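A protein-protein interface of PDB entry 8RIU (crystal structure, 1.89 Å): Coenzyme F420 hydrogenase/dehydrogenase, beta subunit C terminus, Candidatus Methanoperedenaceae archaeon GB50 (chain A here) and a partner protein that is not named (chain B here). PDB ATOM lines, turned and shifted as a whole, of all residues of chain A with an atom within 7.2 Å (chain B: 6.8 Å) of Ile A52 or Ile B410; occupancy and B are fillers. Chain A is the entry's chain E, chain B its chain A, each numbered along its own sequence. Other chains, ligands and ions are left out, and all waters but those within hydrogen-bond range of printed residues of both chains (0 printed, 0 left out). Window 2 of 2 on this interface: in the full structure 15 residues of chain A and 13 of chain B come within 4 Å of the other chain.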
ATOM      1  N   LYS A   6      22.757 -13.806 -12.079  1.00  0.00           N
ATOM      2  CA  LYS A   6      21.396 -13.991 -12.558  1.00  0.00           C
ATOM      3  C   LYS A   6      21.407 -14.279 -14.055  1.00  0.00           C
ATOM      4  O   LYS A   6      22.237 -13.753 -14.804  1.00  0.00           O
ATOM      5  CB  LYS A   6      20.550 -12.749 -12.267  1.00  0.00           C
ATOM      6  CG  LYS A   6      20.251 -12.516 -10.775  1.00  0.00           C
ATOM      7  CD  LYS A   6      19.240 -13.531 -10.261  1.00  0.00           C
ATOM      8  CE  LYS A   6      18.656 -13.125  -8.916  1.00  0.00           C
ATOM      9  NZ  LYS A   6      19.652 -13.200  -7.808  1.00  0.00           N
ATOM     10  N   GLY A   7      20.484 -15.127 -14.484  1.00  0.00           N
ATOM     11  CA  GLY A   7      20.367 -15.448 -15.889  1.00  0.00           C
ATOM     12  C   GLY A   7      19.118 -16.252 -16.160  1.00  0.00           C
ATOM     13  O   GLY A   7      18.517 -16.834 -15.250  1.00  0.00           O
ATOM     14  N   SER A   8      18.734 -16.272 -17.427  1.00  0.00           N
ATOM     15  CA  SER A   8      17.561 -16.994 -17.892  1.00  0.00           C
ATOM     16  C   SER A   8      17.986 -17.978 -18.983  1.00  0.00           C
ATOM     17  O   SER A   8      19.178 -18.182 -19.238  1.00  0.00           O
ATOM     18  CB  SER A   8      16.492 -16.014 -18.387  1.00  0.00           C
ATOM     19  OG  SER A   8      16.807 -15.541 -19.692  1.00  0.00           O
ATOM     20  N   ILE A   9      16.989 -18.587 -19.632  1.00  0.00           N
ATOM     21  CA  ILE A   9      17.264 -19.632 -20.616  1.00  0.00           C
ATOM     22  C   ILE A   9      18.134 -19.095 -21.743  1.00  0.00           C
ATOM     23  O   ILE A   9      18.987 -19.811 -22.281  1.00  0.00           O
ATOM     24  CB  ILE A   9      15.944 -20.224 -21.151  1.00  0.00           C
ATOM     25  CG1 ILE A   9      16.217 -21.287 -22.224  1.00  0.00           C
ATOM     26  CG2 ILE A   9      15.038 -19.129 -21.722  1.00  0.00           C
ATOM     27  CD1 ILE A   9      17.024 -22.472 -21.734  1.00  0.00           C
ATOM     28  N   ASP A  11      20.458 -16.819 -21.599  1.00  0.00           N
ATOM     29  CA  ASP A  11      21.839 -16.811 -21.139  1.00  0.00           C
ATOM     30  C   ASP A  11      22.407 -18.220 -21.102  1.00  0.00           C
ATOM     31  O   ASP A  11      23.569 -18.434 -21.465  1.00  0.00           O
ATOM     32  CB  ASP A  11      21.926 -16.157 -19.766  1.00  0.00           C
ATOM     33  CG  ASP A  11      21.324 -14.777 -19.752  1.00  0.00           C
ATOM     34  OD1 ASP A  11      21.951 -13.854 -20.320  1.00  0.00           O
ATOM     35  OD2 ASP A  11      20.223 -14.618 -19.172  1.00  0.00           O
ATOM     36  N   CYS A  49       9.278 -19.057 -22.365  1.00  0.00           N
ATOM     37  CA  CYS A  49       9.051 -18.902 -20.936  1.00  0.00           C
ATOM     38  C   CYS A  49       9.209 -17.430 -20.559  1.00  0.00           C
ATOM     39  O   CYS A  49       9.699 -16.607 -21.338  1.00  0.00           O
ATOM     40  CB  CYS A  49      10.009 -19.787 -20.130  1.00  0.00           C
ATOM     41  SG  CYS A  49      11.774 -19.573 -20.465  1.00  0.00           S
ATOM     42  N   PHE A  50       8.708 -17.084 -19.373  1.00  0.00           N
ATOM     43  CA  PHE A  50       8.615 -15.649 -19.007  1.00  0.00           C
ATOM     44  C   PHE A  50       9.248 -15.330 -17.649  1.00  0.00           C
ATOM     45  O   PHE A  50       9.005 -14.248 -17.124  1.00  0.00           O
ATOM     46  CB  PHE A  50       7.136 -15.255 -19.075  1.00  0.00           C
ATOM     47  CG  PHE A  50       6.490 -15.520 -20.409  1.00  0.00           C
ATOM     48  CD1 PHE A  50       6.522 -14.569 -21.412  1.00  0.00           C
ATOM     49  CD2 PHE A  50       5.868 -16.729 -20.668  1.00  0.00           C
ATOM     50  CE1 PHE A  50       5.937 -14.815 -22.643  1.00  0.00           C
ATOM     51  CE2 PHE A  50       5.285 -16.975 -21.900  1.00  0.00           C
ATOM     52  CZ  PHE A  50       5.321 -16.019 -22.885  1.00  0.00           C
ATOM     53  N   GLU A  51      10.052 -16.247 -17.104  1.00  0.00           N
ATOM     54  CA  GLU A  51      10.771 -15.965 -15.834  1.00  0.00           C
ATOM     55  C   GLU A  51      11.790 -14.849 -16.096  1.00  0.00           C
ATOM     56  O   GLU A  51      12.367 -14.841 -17.189  1.00  0.00           O
ATOM     57  CB  GLU A  51      11.434 -17.243 -15.301  1.00  0.00           C
ATOM     58  CG  GLU A  51      10.908 -17.732 -13.954  1.00  0.00           C
ATOM     59  CD  GLU A  51      11.640 -18.921 -13.341  1.00  0.00           C
ATOM     60  OE1 GLU A  51      12.376 -19.595 -14.084  1.00  0.00           O
ATOM     61  OE2 GLU A  51      11.478 -19.163 -12.132  1.00  0.00           O
ATOM     62  N   ILE A  52      11.965 -13.921 -15.153  1.00  0.00           N
ATOM     63  CA  ILE A  52      13.016 -12.870 -15.278  1.00  0.00           C
ATOM     64  C   ILE A  52      14.370 -13.561 -15.104  1.00  0.00           C
ATOM     65  O   ILE A  52      15.283 -13.284 -15.900  1.00  0.00           O
ATOM     66  CB  ILE A  52      12.803 -11.757 -14.233  1.00  0.00           C
ATOM     67  CG1 ILE A  52      11.551 -10.931 -14.538  1.00  0.00           C
ATOM     68  CG2 ILE A  52      14.041 -10.883 -14.110  1.00  0.00           C
ATOM     69  CD1 ILE A  52      10.640 -10.735 -13.350  1.00  0.00           C
ATOM     70  N   HIS A  53      14.479 -14.432 -14.099  1.00  0.00           N
ATOM     71  CA  HIS A  53      15.724 -15.214 -13.874  1.00  0.00           C
ATOM     72  C   HIS A  53      15.301 -16.664 -13.638  1.00  0.00           C
ATOM     73  O   HIS A  53      14.246 -16.882 -13.014  1.00  0.00           O
ATOM     74  CB  HIS A  53      16.551 -14.603 -12.739  1.00  0.00           C
ATOM     75  CG  HIS A  53      15.993 -14.829 -11.376  1.00  0.00           C
ATOM     76  ND1 HIS A  53      16.488 -15.789 -10.520  1.00  0.00           N
ATOM     77  CD2 HIS A  53      15.000 -14.223 -10.718  1.00  0.00           C
ATOM     78  CE1 HIS A  53      15.804 -15.756  -9.387  1.00  0.00           C
ATOM     79  NE2 HIS A  53      14.896 -14.813  -9.486  1.00  0.00           N
ATOM     80  N   GLY A  54      16.089 -17.628 -14.121  1.00  0.00           N
ATOM     81  CA  GLY A  54      15.650 -19.032 -14.024  1.00  0.00           C
ATOM     82  C   GLY A  54      16.601 -19.944 -13.273  1.00  0.00           C
ATOM     83  O   GLY A  54      17.802 -19.631 -13.204  1.00  0.00           O
ATOM     84  N   ASP B 405      14.259 -15.437  -6.111  1.00  0.00           N
ATOM     85  CA  ASP B 405      14.810 -14.154  -5.618  1.00  0.00           C
ATOM     86  C   ASP B 405      14.140 -12.960  -6.291  1.00  0.00           C
ATOM     87  O   ASP B 405      13.865 -12.001  -5.585  1.00  0.00           O
ATOM     88  CB  ASP B 405      16.301 -14.069  -5.937  1.00  0.00           C
ATOM     89  CG  ASP B 405      17.222 -13.888  -4.748  1.00  0.00           C
ATOM     90  OD1 ASP B 405      16.759 -14.056  -3.615  1.00  0.00           O
ATOM     91  OD2 ASP B 405      18.403 -13.592  -4.981  1.00  0.00           O
ATOM     92  N   ALA B 406      13.874 -13.038  -7.597  1.00  0.00           N
ATOM     93  CA  ALA B 406      13.403 -11.841  -8.332  1.00  0.00           C
ATOM     94  C   ALA B 406      12.540 -12.167  -9.558  1.00  0.00           C
ATOM     95  O   ALA B 406      12.883 -11.720 -10.654  1.00  0.00           O
ATOM     96  CB  ALA B 406      14.600 -11.022  -8.717  1.00  0.00           C
ATOM     97  N   ASN B 407      11.441 -12.876  -9.359  1.00  0.00           N
ATOM     98  CA  ASN B 407      10.503 -13.121 -10.447  1.00  0.00           C
ATOM     99  C   ASN B 407       9.188 -12.424 -10.081  1.00  0.00           C
ATOM    100  O   ASN B 407       9.037 -11.233 -10.365  1.00  0.00           O
ATOM    101  CB  ASN B 407      10.349 -14.623 -10.712  1.00  0.00           C
ATOM    102  CG  ASN B 407      11.517 -15.192 -11.503  1.00  0.00           C
ATOM    103  OD1 ASN B 407      12.063 -14.527 -12.386  1.00  0.00           O
ATOM    104  ND2 ASN B 407      11.900 -16.430 -11.196  1.00  0.00           N
ATOM    105  N   CYS B 408       8.251 -13.126  -9.450  1.00  0.00           N
ATOM    106  CA  CYS B 408       6.908 -12.550  -9.152  1.00  0.00           C
ATOM    107  C   CYS B 408       7.023 -11.194  -8.436  1.00  0.00           C
ATOM    108  O   CYS B 408       6.304 -10.274  -8.823  1.00  0.00           O
ATOM    109  CB  CYS B 408       6.063 -13.540  -8.352  1.00  0.00           C
ATOM    110  SG  CYS B 408       6.811 -14.106  -6.807  1.00  0.00           S
ATOM    111  N   VAL B 409       7.921 -11.072  -7.466  1.00  0.00           N
ATOM    112  CA  VAL B 409       8.048  -9.810  -6.683  1.00  0.00           C
ATOM    113  C   VAL B 409       8.414  -8.665  -7.634  1.00  0.00           C
ATOM    114  O   VAL B 409       7.929  -7.561  -7.436  1.00  0.00           O
ATOM    115  CB  VAL B 409       9.066  -9.957  -5.538  1.00  0.00           C
ATOM    116  CG1 VAL B 409      10.435 -10.384  -6.039  1.00  0.00           C
ATOM    117  CG2 VAL B 409       9.161  -8.697  -4.694  1.00  0.00           C
ATOM    118  N   ILE B 410       9.224  -8.961  -8.646  1.00  0.00           N
ATOM    119  CA  ILE B 410       9.676  -7.910  -9.599  1.00  0.00           C
ATOM    120  C   ILE B 410       8.516  -7.542 -10.534  1.00  0.00           C
ATOM    121  O   ILE B 410       8.424  -6.379 -10.900  1.00  0.00           O
ATOM    122  CB  ILE B 410      10.919  -8.385 -10.380  1.00  0.00           C
ATOM    123  CG1 ILE B 410      12.056  -8.782  -9.439  1.00  0.00           C
ATOM    124  CG2 ILE B 410      11.367  -7.335 -11.383  1.00  0.00           C
ATOM    125  CD1 ILE B 410      12.401  -7.730  -8.421  1.00  0.00           C
ATOM    126  N   ALA B 411       7.673  -8.510 -10.892  1.00  0.00           N
ATOM    127  CA  ALA B 411       6.560  -8.179 -11.771  1.00  0.00           C
ATOM    128  C   ALA B 411       5.416  -7.502 -11.032  1.00  0.00           C
ATOM    129  O   ALA B 411       4.532  -6.935 -11.680  1.00  0.00           O
ATOM    130  CB  ALA B 411       6.039  -9.438 -12.466  1.00  0.00           C
ATOM    131  N   CYS B 412       5.408  -7.556  -9.708  1.00  0.00           N
ATOM    132  CA  CYS B 412       4.304  -7.013  -8.932  1.00  0.00           C
ATOM    133  C   CYS B 412       4.463  -5.506  -8.772  1.00  0.00           C
ATOM    134  O   CYS B 412       5.522  -5.048  -8.338  1.00  0.00           O
ATOM    135  CB  CYS B 412       4.243  -7.673  -7.556  1.00  0.00           C
ATOM    136  SG  CYS B 412       3.029  -6.917  -6.404  1.00  0.00           S
ATOM    137  N   PRO B 413       3.436  -4.708  -9.089  1.00  0.00           N
ATOM    138  CA  PRO B 413       3.584  -3.253  -8.940  1.00  0.00           C
ATOM    139  C   PRO B 413       3.861  -2.825  -7.509  1.00  0.00           C
ATOM    140  O   PRO B 413       4.471  -1.767  -7.305  1.00  0.00           O
ATOM    141  CB  PRO B 413       2.241  -2.701  -9.451  1.00  0.00           C
ATOM    142  CG  PRO B 413       1.271  -3.813  -9.282  1.00  0.00           C
ATOM    143  CD  PRO B 413       2.066  -5.085  -9.495  1.00  0.00           C
ATOM    144  N   GLY B 415       5.593  -4.834  -5.311  1.00  0.00           N
ATOM    145  CA  GLY B 415       6.728  -5.582  -4.786  1.00  0.00           C
ATOM    146  C   GLY B 415       6.394  -6.464  -3.603  1.00  0.00           C
ATOM    147  O   GLY B 415       7.178  -6.543  -2.650  1.00  0.00           O
ATOM    148  N   LEU B 416       5.258  -7.146  -3.647  1.00  0.00           N
ATOM    149  CA  LEU B 416       4.821  -7.934  -2.502  1.00  0.00           C
ATOM    150  C   LEU B 416       5.675  -9.190  -2.332  1.00  0.00           C
ATOM    151  O   LEU B 416       6.098  -9.802  -3.322  1.00  0.00           O
ATOM    152  CB  LEU B 416       3.354  -8.313  -2.664  1.00  0.00           C
ATOM    153  CG  LEU B 416       2.377  -7.131  -2.661  1.00  0.00           C
ATOM    154  CD1 LEU B 416       0.977  -7.630  -2.510  1.00  0.00           C
ATOM    155  CD2 LEU B 416       2.681  -6.117  -1.564  1.00  0.00           C
ATOM    156  N   ARG B 445      -0.145  -9.594 -12.778  1.00  0.00           N
ATOM    157  CA  ARG B 445       1.159  -9.620 -13.493  1.00  0.00           C
ATOM    158  C   ARG B 445       2.059 -10.704 -12.886  1.00  0.00           C
ATOM    159  O   ARG B 445       2.748 -11.383 -13.645  1.00  0.00           O
ATOM    160  CB  ARG B 445       1.817  -8.241 -13.437  1.00  0.00           C
ATOM    161  CG  ARG B 445       1.178  -7.184 -14.324  1.00  0.00           C
ATOM    162  CD  ARG B 445       2.186  -6.174 -14.842  1.00  0.00           C
ATOM    163  NE  ARG B 445       3.056  -5.637 -13.810  1.00  0.00           N
ATOM    164  CZ  ARG B 445       3.097  -4.364 -13.440  1.00  0.00           C
ATOM    165  NH1 ARG B 445       2.386  -3.463 -14.091  1.00  0.00           N
ATOM    166  NH2 ARG B 445       3.847  -3.996 -12.420  1.00  0.00           N
ATOM    167  N   VAL B 449       4.941 -14.436 -14.769  1.00  0.00           N
ATOM    168  CA  VAL B 449       6.374 -14.700 -14.721  1.00  0.00           C
ATOM    169  C   VAL B 449       6.712 -15.916 -13.863  1.00  0.00           C
ATOM    170  O   VAL B 449       7.901 -16.216 -13.658  1.00  0.00           O
ATOM    171  CB  VAL B 449       7.137 -13.461 -14.212  1.00  0.00           C
ATOM    172  CG1 VAL B 449       6.944 -12.278 -15.168  1.00  0.00           C
ATOM    173  CG2 VAL B 449       6.680 -13.094 -12.809  1.00  0.00           C
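Val B449 touches Phe A50 (CG1 to O, 3.5 Å). Glu A51 touches Val B449. Ala B406 touches Ile A52 (O to CB, 3.6 Å). Ile A52 touches Ile B410 (CD1 to CB, 3.8 Å).
Asp A11 touches none of the printed residues of chain B. Cys A49 touches none of the printed residues of chain B. Of the printed residues of chain B, Phe A50 touches Val B449 (3.5 Å). Of the printed residues of chain B, Glu A51 touches Asn B407 (2.9 Å) and Val B449 (3.4 Å). Ile A52 touches three residues of chain B. Of the printed residues of chain A, Asp B405 touches Lys A6 (3.1 Å) and His A53 (3.5 Å). Of the printed residues of chain A, Asn B407 touches Glu A51 (2.9 Å), Ile A52 (2.8 Å) and His A53 (3.0 Å). Ile B410 touches just one residue of chain A: Ile A52. The nearest residue of chain B that does not touch Ile A52 is Val B449 (4.4 Å). The nearest residue of chain A that does not touch Ile B410 is His A53 (6.3 Å).
The side-chain amide nitrogen of Asn B407 is in hydrogen-bond range of the side-chain carboxylate of Glu A51 (2.9 Å). The side-chain amide oxygen of Asn B407 lies within hydrogen-bond range of the backbone NH of Ile A52, 2.8 Å away. OD1 of Asn B407 lies within hydrogen-bond range of N of His A53. The side-chain amino group of Lys A6 is in salt-bridge range of the side-chain carboxylate of Asp B405 (3.1 Å). N of Asp B405 lies within hydrogen-bond range of NE2 of His A53 (3.5 Å). N of Ala B406 is in hydrogen-bond range of NE2 of His A53, at 2.8 Å.
Among the printed residues, 10 pairs touch across the chains. Among the printed residues, Asp or Glu carboxylates within 4 Å of a Lys or Arg side-chain nitrogen of the other chain: Lys A6 with Asp B405 (3.1 Å).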
